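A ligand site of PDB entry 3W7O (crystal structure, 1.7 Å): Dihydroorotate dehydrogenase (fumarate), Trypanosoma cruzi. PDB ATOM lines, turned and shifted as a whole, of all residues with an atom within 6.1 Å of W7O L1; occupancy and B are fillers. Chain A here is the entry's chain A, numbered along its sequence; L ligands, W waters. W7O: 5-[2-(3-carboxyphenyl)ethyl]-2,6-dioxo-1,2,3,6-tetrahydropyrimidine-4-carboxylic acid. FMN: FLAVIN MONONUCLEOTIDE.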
ATOM      1  N   ALA A  20      14.833  16.437  33.040  1.00  0.00           N
ATOM      2  CA  ALA A  20      15.735  15.552  32.359  1.00  0.00           C
ATOM      3  C   ALA A  20      17.181  15.923  32.685  1.00  0.00           C
ATOM      4  O   ALA A  20      17.514  17.079  32.780  1.00  0.00           O
ATOM      5  CB  ALA A  20      15.519  15.585  30.836  1.00  0.00           C
ATOM      6  N   LYS A  44      17.298  10.407  31.385  1.00  0.00           N
ATOM      7  CA  LYS A  44      18.294  11.248  30.806  1.00  0.00           C
ATOM      8  C   LYS A  44      18.199  11.276  29.278  1.00  0.00           C
ATOM      9  O   LYS A  44      18.114  10.236  28.644  1.00  0.00           O
ATOM     10  CB  LYS A  44      19.647  10.669  31.198  1.00  0.00           C
ATOM     11  CG  LYS A  44      20.887  11.401  30.571  1.00  0.00           C
ATOM     12  CD  LYS A  44      21.065  12.864  30.910  1.00  0.00           C
ATOM     13  CE  LYS A  44      22.084  13.615  30.020  1.00  0.00           C
ATOM     14  NZ  LYS A  44      22.455  15.123  30.273  1.00  0.00           N
ATOM     15  N   SER A  45      18.298  12.477  28.711  1.00  0.00           N
ATOM     16  CA  SER A  45      18.383  12.666  27.246  1.00  0.00           C
ATOM     17  C   SER A  45      19.430  11.755  26.710  1.00  0.00           C
ATOM     18  O   SER A  45      20.556  11.780  27.139  1.00  0.00           O
ATOM     19  CB  SER A  45      18.641  14.074  26.783  1.00  0.00           C
ATOM     20  OG  SER A  45      17.574  14.894  27.180  1.00  0.00           O
ATOM     21  N   ARG A  51      27.561   7.911  25.533  1.00  0.00           N
ATOM     22  CA  ARG A  51      28.496   8.981  25.606  1.00  0.00           C
ATOM     23  C   ARG A  51      29.035   9.181  27.007  1.00  0.00           C
ATOM     24  O   ARG A  51      28.317   9.119  27.944  1.00  0.00           O
ATOM     25  CB  ARG A  51      27.859  10.296  25.215  1.00  0.00           C
ATOM     26  CG  ARG A  51      27.437  10.362  23.790  1.00  0.00           C
ATOM     27  CD  ARG A  51      26.705  11.622  23.463  1.00  0.00           C
ATOM     28  NE  ARG A  51      27.381  12.846  23.845  1.00  0.00           N
ATOM     29  CZ  ARG A  51      28.168  13.520  23.024  1.00  0.00           C
ATOM     30  NH1 ARG A  51      28.384  13.031  21.826  1.00  0.00           N
ATOM     31  NH2 ARG A  51      28.725  14.607  23.421  1.00  0.00           N
ATOM     32  N   ASN A  54      31.418  15.431  28.723  1.00  0.00           N
ATOM     33  CA  ASN A  54      32.525  16.330  28.901  1.00  0.00           C
ATOM     34  C   ASN A  54      33.373  16.024  30.141  1.00  0.00           C
ATOM     35  O   ASN A  54      33.018  15.381  31.037  1.00  0.00           O
ATOM     36  CB  ASN A  54      32.075  17.800  28.933  1.00  0.00           C
ATOM     37  CG  ASN A  54      31.592  18.334  27.578  1.00  0.00           C
ATOM     38  OD1 ASN A  54      31.972  17.845  26.585  1.00  0.00           O
ATOM     39  ND2 ASN A  54      30.758  19.357  27.596  1.00  0.00           N
ATOM     40  N   ASN A  68      26.027  24.130  34.100  1.00  0.00           N
ATOM     41  CA  ASN A  68      26.505  22.825  33.616  1.00  0.00           C
ATOM     42  C   ASN A  68      26.854  22.882  32.112  1.00  0.00           C
ATOM     43  O   ASN A  68      26.185  23.494  31.294  1.00  0.00           O
ATOM     44  CB  ASN A  68      25.495  21.721  33.906  1.00  0.00           C
ATOM     45  CG  ASN A  68      24.448  21.585  32.824  1.00  0.00           C
ATOM     46  OD1 ASN A  68      24.672  20.968  31.757  1.00  0.00           O
ATOM     47  ND2 ASN A  68      23.331  22.146  33.084  1.00  0.00           N
ATOM     48  N   SER A  69      27.878  22.117  31.757  1.00  0.00           N
ATOM     49  CA  SER A  69      28.161  21.727  30.386  1.00  0.00           C
ATOM     50  C   SER A  69      28.487  20.255  30.439  1.00  0.00           C
ATOM     51  O   SER A  69      29.618  19.821  30.238  1.00  0.00           O
ATOM     52  CB  SER A  69      29.299  22.504  29.762  1.00  0.00           C
ATOM     53  OG  SER A  69      29.540  22.012  28.474  1.00  0.00           O
ATOM     54  N   MET A  70      27.465  19.442  30.638  1.00  0.00           N
ATOM     55  CA  MET A  70      27.706  18.051  30.873  1.00  0.00           C
ATOM     56  C   MET A  70      28.190  17.344  29.597  1.00  0.00           C
ATOM     57  O   MET A  70      28.938  16.351  29.662  1.00  0.00           O
ATOM     58  CB  MET A  70      26.422  17.392  31.282  1.00  0.00           C
ATOM     59  CG  MET A  70      25.715  17.850  32.548  1.00  0.00           C
ATOM     60  SD  MET A  70      26.758  17.804  33.981  1.00  0.00           S
ATOM     61  CE  MET A  70      26.758  16.080  34.346  1.00  0.00           C
ATOM     62  N   GLY A  71      27.718  17.765  28.422  1.00  0.00           N
ATOM     63  CA  GLY A  71      28.110  17.138  27.139  1.00  0.00           C
ATOM     64  C   GLY A  71      27.259  15.923  26.813  1.00  0.00           C
ATOM     65  O   GLY A  71      27.767  14.998  26.186  1.00  0.00           O
ATOM     66  N   LEU A  72      26.055  15.847  27.337  1.00  0.00           N
ATOM     67  CA  LEU A  72      25.169  14.770  27.033  1.00  0.00           C
ATOM     68  C   LEU A  72      25.745  13.369  27.346  1.00  0.00           C
ATOM     69  O   LEU A  72      25.592  12.342  26.593  1.00  0.00           O
ATOM     70  CB  LEU A  72      24.708  14.897  25.578  1.00  0.00           C
ATOM     71  CG  LEU A  72      23.388  14.428  25.067  1.00  0.00           C
ATOM     72  CD1 LEU A  72      22.219  14.565  25.980  1.00  0.00           C
ATOM     73  CD2 LEU A  72      23.219  15.067  23.661  1.00  0.00           C
ATOM     74  N   PRO A  73      26.341  13.207  28.525  1.00  0.00           N
ATOM     75  CA  PRO A  73      26.691  11.848  28.946  1.00  0.00           C
ATOM     76  C   PRO A  73      25.462  10.942  29.164  1.00  0.00           C
ATOM     77  O   PRO A  73      24.439  11.404  29.730  1.00  0.00           O
ATOM     78  CB  PRO A  73      27.359  12.078  30.312  1.00  0.00           C
ATOM     79  CG  PRO A  73      26.738  13.290  30.842  1.00  0.00           C
ATOM     80  CD  PRO A  73      26.416  14.173  29.660  1.00  0.00           C
ATOM     81  N   SER A 100      17.719  13.048  22.627  1.00  0.00           N
ATOM     82  CA  SER A 100      18.369  14.248  22.179  1.00  0.00           C
ATOM     83  C   SER A 100      19.470  13.876  21.159  1.00  0.00           C
ATOM     84  O   SER A 100      20.694  14.104  21.394  1.00  0.00           O
ATOM     85  CB  SER A 100      18.895  14.974  23.429  1.00  0.00           C
ATOM     86  OG  SER A 100      19.588  16.064  23.060  1.00  0.00           O
ATOM     87  N   LEU A 102      21.889  14.006  17.948  1.00  0.00           N
ATOM     88  CA  LEU A 102      22.770  15.035  17.443  1.00  0.00           C
ATOM     89  C   LEU A 102      22.503  15.478  15.991  1.00  0.00           C
ATOM     90  O   LEU A 102      23.183  16.405  15.493  1.00  0.00           O
ATOM     91  CB  LEU A 102      24.247  14.578  17.610  1.00  0.00           C
ATOM     92  CG  LEU A 102      24.592  14.200  19.100  1.00  0.00           C
ATOM     93  CD1 LEU A 102      26.061  13.957  19.257  1.00  0.00           C
ATOM     94  CD2 LEU A 102      24.186  15.295  19.942  1.00  0.00           C
ATOM     95  N   ASN A 128      14.168  16.551  23.027  1.00  0.00           N
ATOM     96  CA  ASN A 128      14.883  17.729  23.448  1.00  0.00           C
ATOM     97  C   ASN A 128      15.378  18.485  22.207  1.00  0.00           C
ATOM     98  O   ASN A 128      16.283  18.033  21.485  1.00  0.00           O
ATOM     99  CB  ASN A 128      16.098  17.258  24.255  1.00  0.00           C
ATOM    100  CG  ASN A 128      16.908  18.407  24.813  1.00  0.00           C
ATOM    101  OD1 ASN A 128      16.554  19.505  24.733  1.00  0.00           O
ATOM    102  ND2 ASN A 128      17.950  18.030  25.506  1.00  0.00           N
ATOM    103  N   SER A 130      16.468  21.688  22.599  1.00  0.00           N
ATOM    104  CA  SER A 130      17.383  22.664  23.163  1.00  0.00           C
ATOM    105  C   SER A 130      18.720  22.042  23.226  1.00  0.00           C
ATOM    106  O   SER A 130      19.178  21.678  24.251  1.00  0.00           O
ATOM    107  CB  SER A 130      16.940  23.154  24.559  1.00  0.00           C
ATOM    108  OG  SER A 130      15.649  22.659  24.917  1.00  0.00           O
ATOM    109  N   CYS A 131      19.224  21.724  22.057  1.00  0.00           N
ATOM    110  CA  CYS A 131      20.428  20.972  21.955  1.00  0.00           C
ATOM    111  C   CYS A 131      21.199  21.346  20.685  1.00  0.00           C
ATOM    112  O   CYS A 131      20.662  21.966  19.753  1.00  0.00           O
ATOM    113  CB  CYS A 131      19.997  19.513  21.875  1.00  0.00           C
ATOM    114  SG  CYS A 131      19.054  19.202  20.399  1.00  0.00           S
ATOM    115  N   PRO A 132      22.435  20.853  20.571  1.00  0.00           N
ATOM    116  CA  PRO A 132      23.211  21.178  19.361  1.00  0.00           C
ATOM    117  C   PRO A 132      22.827  20.453  18.117  1.00  0.00           C
ATOM    118  O   PRO A 132      22.379  19.366  18.176  1.00  0.00           O
ATOM    119  CB  PRO A 132      24.632  20.748  19.701  1.00  0.00           C
ATOM    120  CG  PRO A 132      24.643  20.330  21.082  1.00  0.00           C
ATOM    121  CD  PRO A 132      23.281  20.419  21.702  1.00  0.00           C
ATOM    122  N   LYS A 165      11.013  19.569  24.625  1.00  0.00           N
ATOM    123  CA  LYS A 165      11.694  20.364  25.669  1.00  0.00           C
ATOM    124  C   LYS A 165      12.315  21.573  24.972  1.00  0.00           C
ATOM    125  O   LYS A 165      13.123  21.449  24.052  1.00  0.00           O
ATOM    126  CB  LYS A 165      12.801  19.511  26.271  1.00  0.00           C
ATOM    127  CG  LYS A 165      13.642  20.192  27.319  1.00  0.00           C
ATOM    128  CD  LYS A 165      12.882  20.449  28.627  1.00  0.00           C
ATOM    129  CE  LYS A 165      13.801  20.867  29.763  1.00  0.00           C
ATOM    130  NZ  LYS A 165      14.602  19.801  30.307  1.00  0.00           N
ATOM    131  N   ASN A 195      14.394  24.551  29.311  1.00  0.00           N
ATOM    132  CA  ASN A 195      15.756  24.077  29.493  1.00  0.00           C
ATOM    133  C   ASN A 195      16.618  25.228  30.078  1.00  0.00           C
ATOM    134  O   ASN A 195      16.119  26.250  30.344  1.00  0.00           O
ATOM    135  CB  ASN A 195      16.308  23.598  28.133  1.00  0.00           C
ATOM    136  CG  ASN A 195      17.308  22.461  28.260  1.00  0.00           C
ATOM    137  OD1 ASN A 195      18.130  22.509  29.060  1.00  0.00           O
ATOM    138  ND2 ASN A 195      17.156  21.461  27.457  1.00  0.00           N
ATOM    139  N   SER A 196      17.886  24.948  30.323  1.00  0.00           N
ATOM    140  CA  SER A 196      18.708  25.947  31.001  1.00  0.00           C
ATOM    141  C   SER A 196      18.814  27.225  30.203  1.00  0.00           C
ATOM    142  O   SER A 196      18.651  27.226  29.038  1.00  0.00           O
ATOM    143  CB  SER A 196      20.131  25.482  31.270  1.00  0.00           C
ATOM    144  OG  SER A 196      20.545  24.522  30.477  1.00  0.00           O
ATOM    145  N   LYS A 215      34.193  24.447  27.607  1.00  0.00           N
ATOM    146  CA  LYS A 215      33.689  25.683  26.981  1.00  0.00           C
ATOM    147  C   LYS A 215      34.194  26.926  27.690  1.00  0.00           C
ATOM    148  O   LYS A 215      33.514  27.920  27.722  1.00  0.00           O
ATOM    149  CB  LYS A 215      32.126  25.651  26.868  1.00  0.00           C
ATOM    150  CG  LYS A 215      31.567  24.632  25.861  1.00  0.00           C
ATOM    151  CD  LYS A 215      30.044  24.563  25.967  1.00  0.00           C
ATOM    152  CE  LYS A 215      29.395  25.901  25.767  1.00  0.00           C
ATOM    153  NZ  LYS A 215      27.910  25.796  25.481  1.00  0.00           N
ATOM    154  N   GLY A 220      25.041  26.091  30.839  1.00  0.00           N
ATOM    155  CA  GLY A 220      23.624  26.431  31.060  1.00  0.00           C
ATOM    156  C   GLY A 220      23.283  26.629  32.503  1.00  0.00           C
ATOM    157  O   GLY A 220      23.759  25.908  33.388  1.00  0.00           O
HETATM  158  OAA W7O L   1      26.763  18.581  24.282  1.00  0.00           O
HETATM  159  CAO W7O L   1      26.518  19.799  24.558  1.00  0.00           C
HETATM  160  OAE W7O L   1      27.399  20.717  24.343  1.00  0.00           O
HETATM  161  CAR W7O L   1      25.247  20.205  24.913  1.00  0.00           C
HETATM  162  CAJ W7O L   1      24.192  19.238  24.985  1.00  0.00           C
HETATM  163  CAI W7O L   1      25.071  21.558  25.186  1.00  0.00           C
HETATM  164  CAG W7O L   1      23.845  22.066  25.540  1.00  0.00           C
HETATM  165  CAH W7O L   1      22.765  21.130  25.612  1.00  0.00           C
HETATM  166  CAQ W7O L   1      22.944  19.741  25.319  1.00  0.00           C
HETATM  167  CAK W7O L   1      21.901  18.874  25.460  1.00  0.00           C
HETATM  168  CAL W7O L   1      21.800  18.167  26.856  1.00  0.00           C
HETATM  169  CAS W7O L   1      21.664  19.103  27.939  1.00  0.00           C
HETATM  170  CAV W7O L   1      20.475  19.869  28.061  1.00  0.00           C
HETATM  171  OAD W7O L   1      19.516  19.705  27.296  1.00  0.00           O
HETATM  172  NAN W7O L   1      20.401  20.791  29.112  1.00  0.00           N
HETATM  173  CAU W7O L   1      21.481  21.064  29.962  1.00  0.00           C
HETATM  174  OAC W7O L   1      21.402  21.922  30.853  1.00  0.00           O
HETATM  175  NAM W7O L   1      22.607  20.248  29.793  1.00  0.00           N
HETATM  176  CAT W7O L   1      22.695  19.296  28.812  1.00  0.00           C
HETATM  177  CAP W7O L   1      24.043  18.622  28.744  1.00  0.00           C
HETATM  178  OAF W7O L   1      24.988  19.457  28.737  1.00  0.00           O
HETATM  179  OAB W7O L   1      24.147  17.398  28.704  1.00  0.00           O
HETATM  180  N1  FMN L   2      17.673  19.014  30.007  1.00  0.00           N
HETATM  181  C2  FMN L   2      17.406  18.145  29.028  1.00  0.00           C
HETATM  182  O2  FMN L   2      16.295  18.267  28.428  1.00  0.00           O
HETATM  183  N3  FMN L   2      18.137  17.003  28.805  1.00  0.00           N
HETATM  184  C4  FMN L   2      19.191  16.724  29.597  1.00  0.00           C
HETATM  185  O4  FMN L   2      19.957  15.714  29.432  1.00  0.00           O
HETATM  186  C4A FMN L   2      19.590  17.688  30.641  1.00  0.00           C
HETATM  187  N5  FMN L   2      20.695  17.440  31.392  1.00  0.00           N
HETATM  188  C5A FMN L   2      20.919  18.270  32.472  1.00  0.00           C
HETATM  189  C6  FMN L   2      21.928  17.898  33.417  1.00  0.00           C
HETATM  190  C7  FMN L   2      22.164  18.727  34.466  1.00  0.00           C
HETATM  191  C7M FMN L   2      23.263  18.389  35.458  1.00  0.00           C
HETATM  192  C8  FMN L   2      21.329  19.872  34.714  1.00  0.00           C
HETATM  193  C8M FMN L   2      21.606  20.770  35.922  1.00  0.00           C
HETATM  194  C9  FMN L   2      20.275  20.193  33.841  1.00  0.00           C
HETATM  195  C9A FMN L   2      20.054  19.404  32.721  1.00  0.00           C
HETATM  196  N10 FMN L   2      19.026  19.708  31.817  1.00  0.00           N
HETATM  197  C10 FMN L   2      18.746  18.854  30.819  1.00  0.00           C
HETATM  198  C1' FMN L   2      18.139  20.851  32.016  1.00  0.00           C
HETATM  199  C2' FMN L   2      17.131  20.597  33.104  1.00  0.00           C
HETATM  200  O2' FMN L   2      16.286  19.586  32.618  1.00  0.00           O
HETATM  201  C3' FMN L   2      16.367  21.827  33.339  1.00  0.00           C
HETATM  202  O3' FMN L   2      15.651  22.164  32.124  1.00  0.00           O
HETATM  203  C4' FMN L   2      17.181  23.061  33.786  1.00  0.00           C
HETATM  204  O4' FMN L   2      18.161  22.612  34.722  1.00  0.00           O
HETATM  205  C5' FMN L   2      16.230  24.098  34.469  1.00  0.00           C
HETATM  206  O5' FMN L   2      15.542  23.652  35.646  1.00  0.00           O
HETATM  207  P   FMN L   2      16.064  23.953  37.127  1.00  0.00           P
HETATM  208  O1P FMN L   2      15.121  23.173  38.014  1.00  0.00           O
HETATM  209  O2P FMN L   2      16.097  25.456  37.262  1.00  0.00           O
HETATM  210  O3P FMN L   2      17.490  23.379  37.176  1.00  0.00           O
HETATM  211  O   HOH W   1      29.769  20.656  25.187  1.00  0.00           O
HETATM  212  O   HOH W   2      27.609  20.794  27.377  1.00  0.00           O
HETATM  213  O   HOH W   3      24.845  22.476  28.924  1.00  0.00           O
HETATM  214  O   HOH W   4      27.103  22.690  22.047  1.00  0.00           O
HETATM  215  O   HOH W   5      29.224  18.266  22.021  1.00  0.00           O
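The side-chain amide oxygen (OD1) of Asn 195 sits at hydrogen-bond distance from the side-chain hydroxyl (OG) of Ser 196. The backbone carbonyl oxygen (O) of Leu 72 sits at hydrogen-bond distance from the guanidinium group (NE) of Arg 51. The backbone carbonyl oxygen of Lys 165 lies within hydrogen-bond range of the side-chain hydroxyl of Ser 130. The side-chain amide oxygen (OD1) of Asn 128 lies within hydrogen-bond range of the side-chain amide nitrogen (ND2) of Asn 195 (3.4 Å). N of Ser 130 sits at hydrogen-bond distance from OD1 of Asn 128 (3.1 Å). The backbone carbonyl oxygen (O) of Met 70 is in hydrogen-bond range of the backbone NH (N) of Asn 54. OD1 of Asn 68 sits at hydrogen-bond distance from N of Met 70. SG of Cys 131 lies within hydrogen-bond range of O of Asn 128.
A nitrogen (N1) of FMN L2 sits close to a nitrogen (NAN) of W7O L1 (3.4 Å).
C of Ser 69 touches OAF of W7O L1, at 3.97 Å. O of Ser 130 touches OAD of W7O L1 (3.6 Å). Pro 132 touches W7O L1. Hydrophobic or aromatic side chains that line W7O L1: Met 70, Leu 72 and Pro 132. 11 residues have an atom within 4 Å of W7O L1: Lys 44, Asn 68, Ser 69, Met 70, Gly 71, Leu 72, Asn 128, Ser 130, Pro 132, Asn 195 and Ser 196. Along chain A the residues within 4 Å of W7O L1 span positions 44 to 196. The nearest printed residue that does not touch W7O L1 is Pro 73 (4.1 Å).
OG of Ser 45 is in hydrogen-bond range of N3 of FMN L2 (2.7 Å). ND2 of Asn 128 sits at hydrogen-bond distance from O2 of FMN L2 (3.4 Å). A nitrogen (NAM) of W7O L1 lies within hydrogen-bond range of the side-chain amide oxygen (OD1) of Asn 68 (2.9 Å). OAD of W7O L1 is in hydrogen-bond range of ND2 of Asn 128. The side-chain amide nitrogen of Asn 195 lies within hydrogen-bond range of an oxygen (O2) of FMN L2, at 3.4 Å. An oxygen (O2') of FMN L2 sits at hydrogen-bond distance from the backbone carbonyl oxygen (O) of Ala 20. N of Met 70 is in hydrogen-bond range of OAF of W7O L1 (3.1 Å). OD1 of Asn 195 is in hydrogen-bond range of NAN of W7O L1 (2.8 Å). The side-chain hydroxyl (OG) of Ser 196 is in hydrogen-bond range of an oxygen (OAC) of W7O L1 (2.8 Å). The backbone NH (N) of Gly 71 sits at hydrogen-bond distance from an oxygen (OAF) of W7O L1 (3.2 Å). O2' of FMN L2 is in hydrogen-bond range of N of Ala 20, 3.5 Å away. OAB of W7O L1 lies within salt-bridge range of NZ of Lys 44 (3.2 Å). The side-chain amino group of Lys 165 is in hydrogen-bond range of an oxygen (O2') of FMN L2, at 2.9 Å. OAB of W7O L1 lies within hydrogen-bond range of N of Leu 72, 2.8 Å away. NZ of Lys 44 sits at hydrogen-bond distance from O4 of FMN L2, 2.7 Å away.
Water W1 lies within hydrogen-bond range of an oxygen (OAE) of W7O L1 (2.5 Å) and the side-chain amide nitrogen of Asn 54 (2.9 Å). Water W3 lies within hydrogen-bond range of O of Asn 68 (2.9 Å) and OAF of W7O L1 (3.0 Å). Water W2 lies within hydrogen-bond range of the side-chain hydroxyl (OG) of Ser 69 (2.5 Å), an oxygen (OAE) of W7O L1 (3.0 Å), the backbone NH (N) of Gly 71 (3.2 Å) and the side-chain amide nitrogen (ND2) of Asn 54 (3.5 Å).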
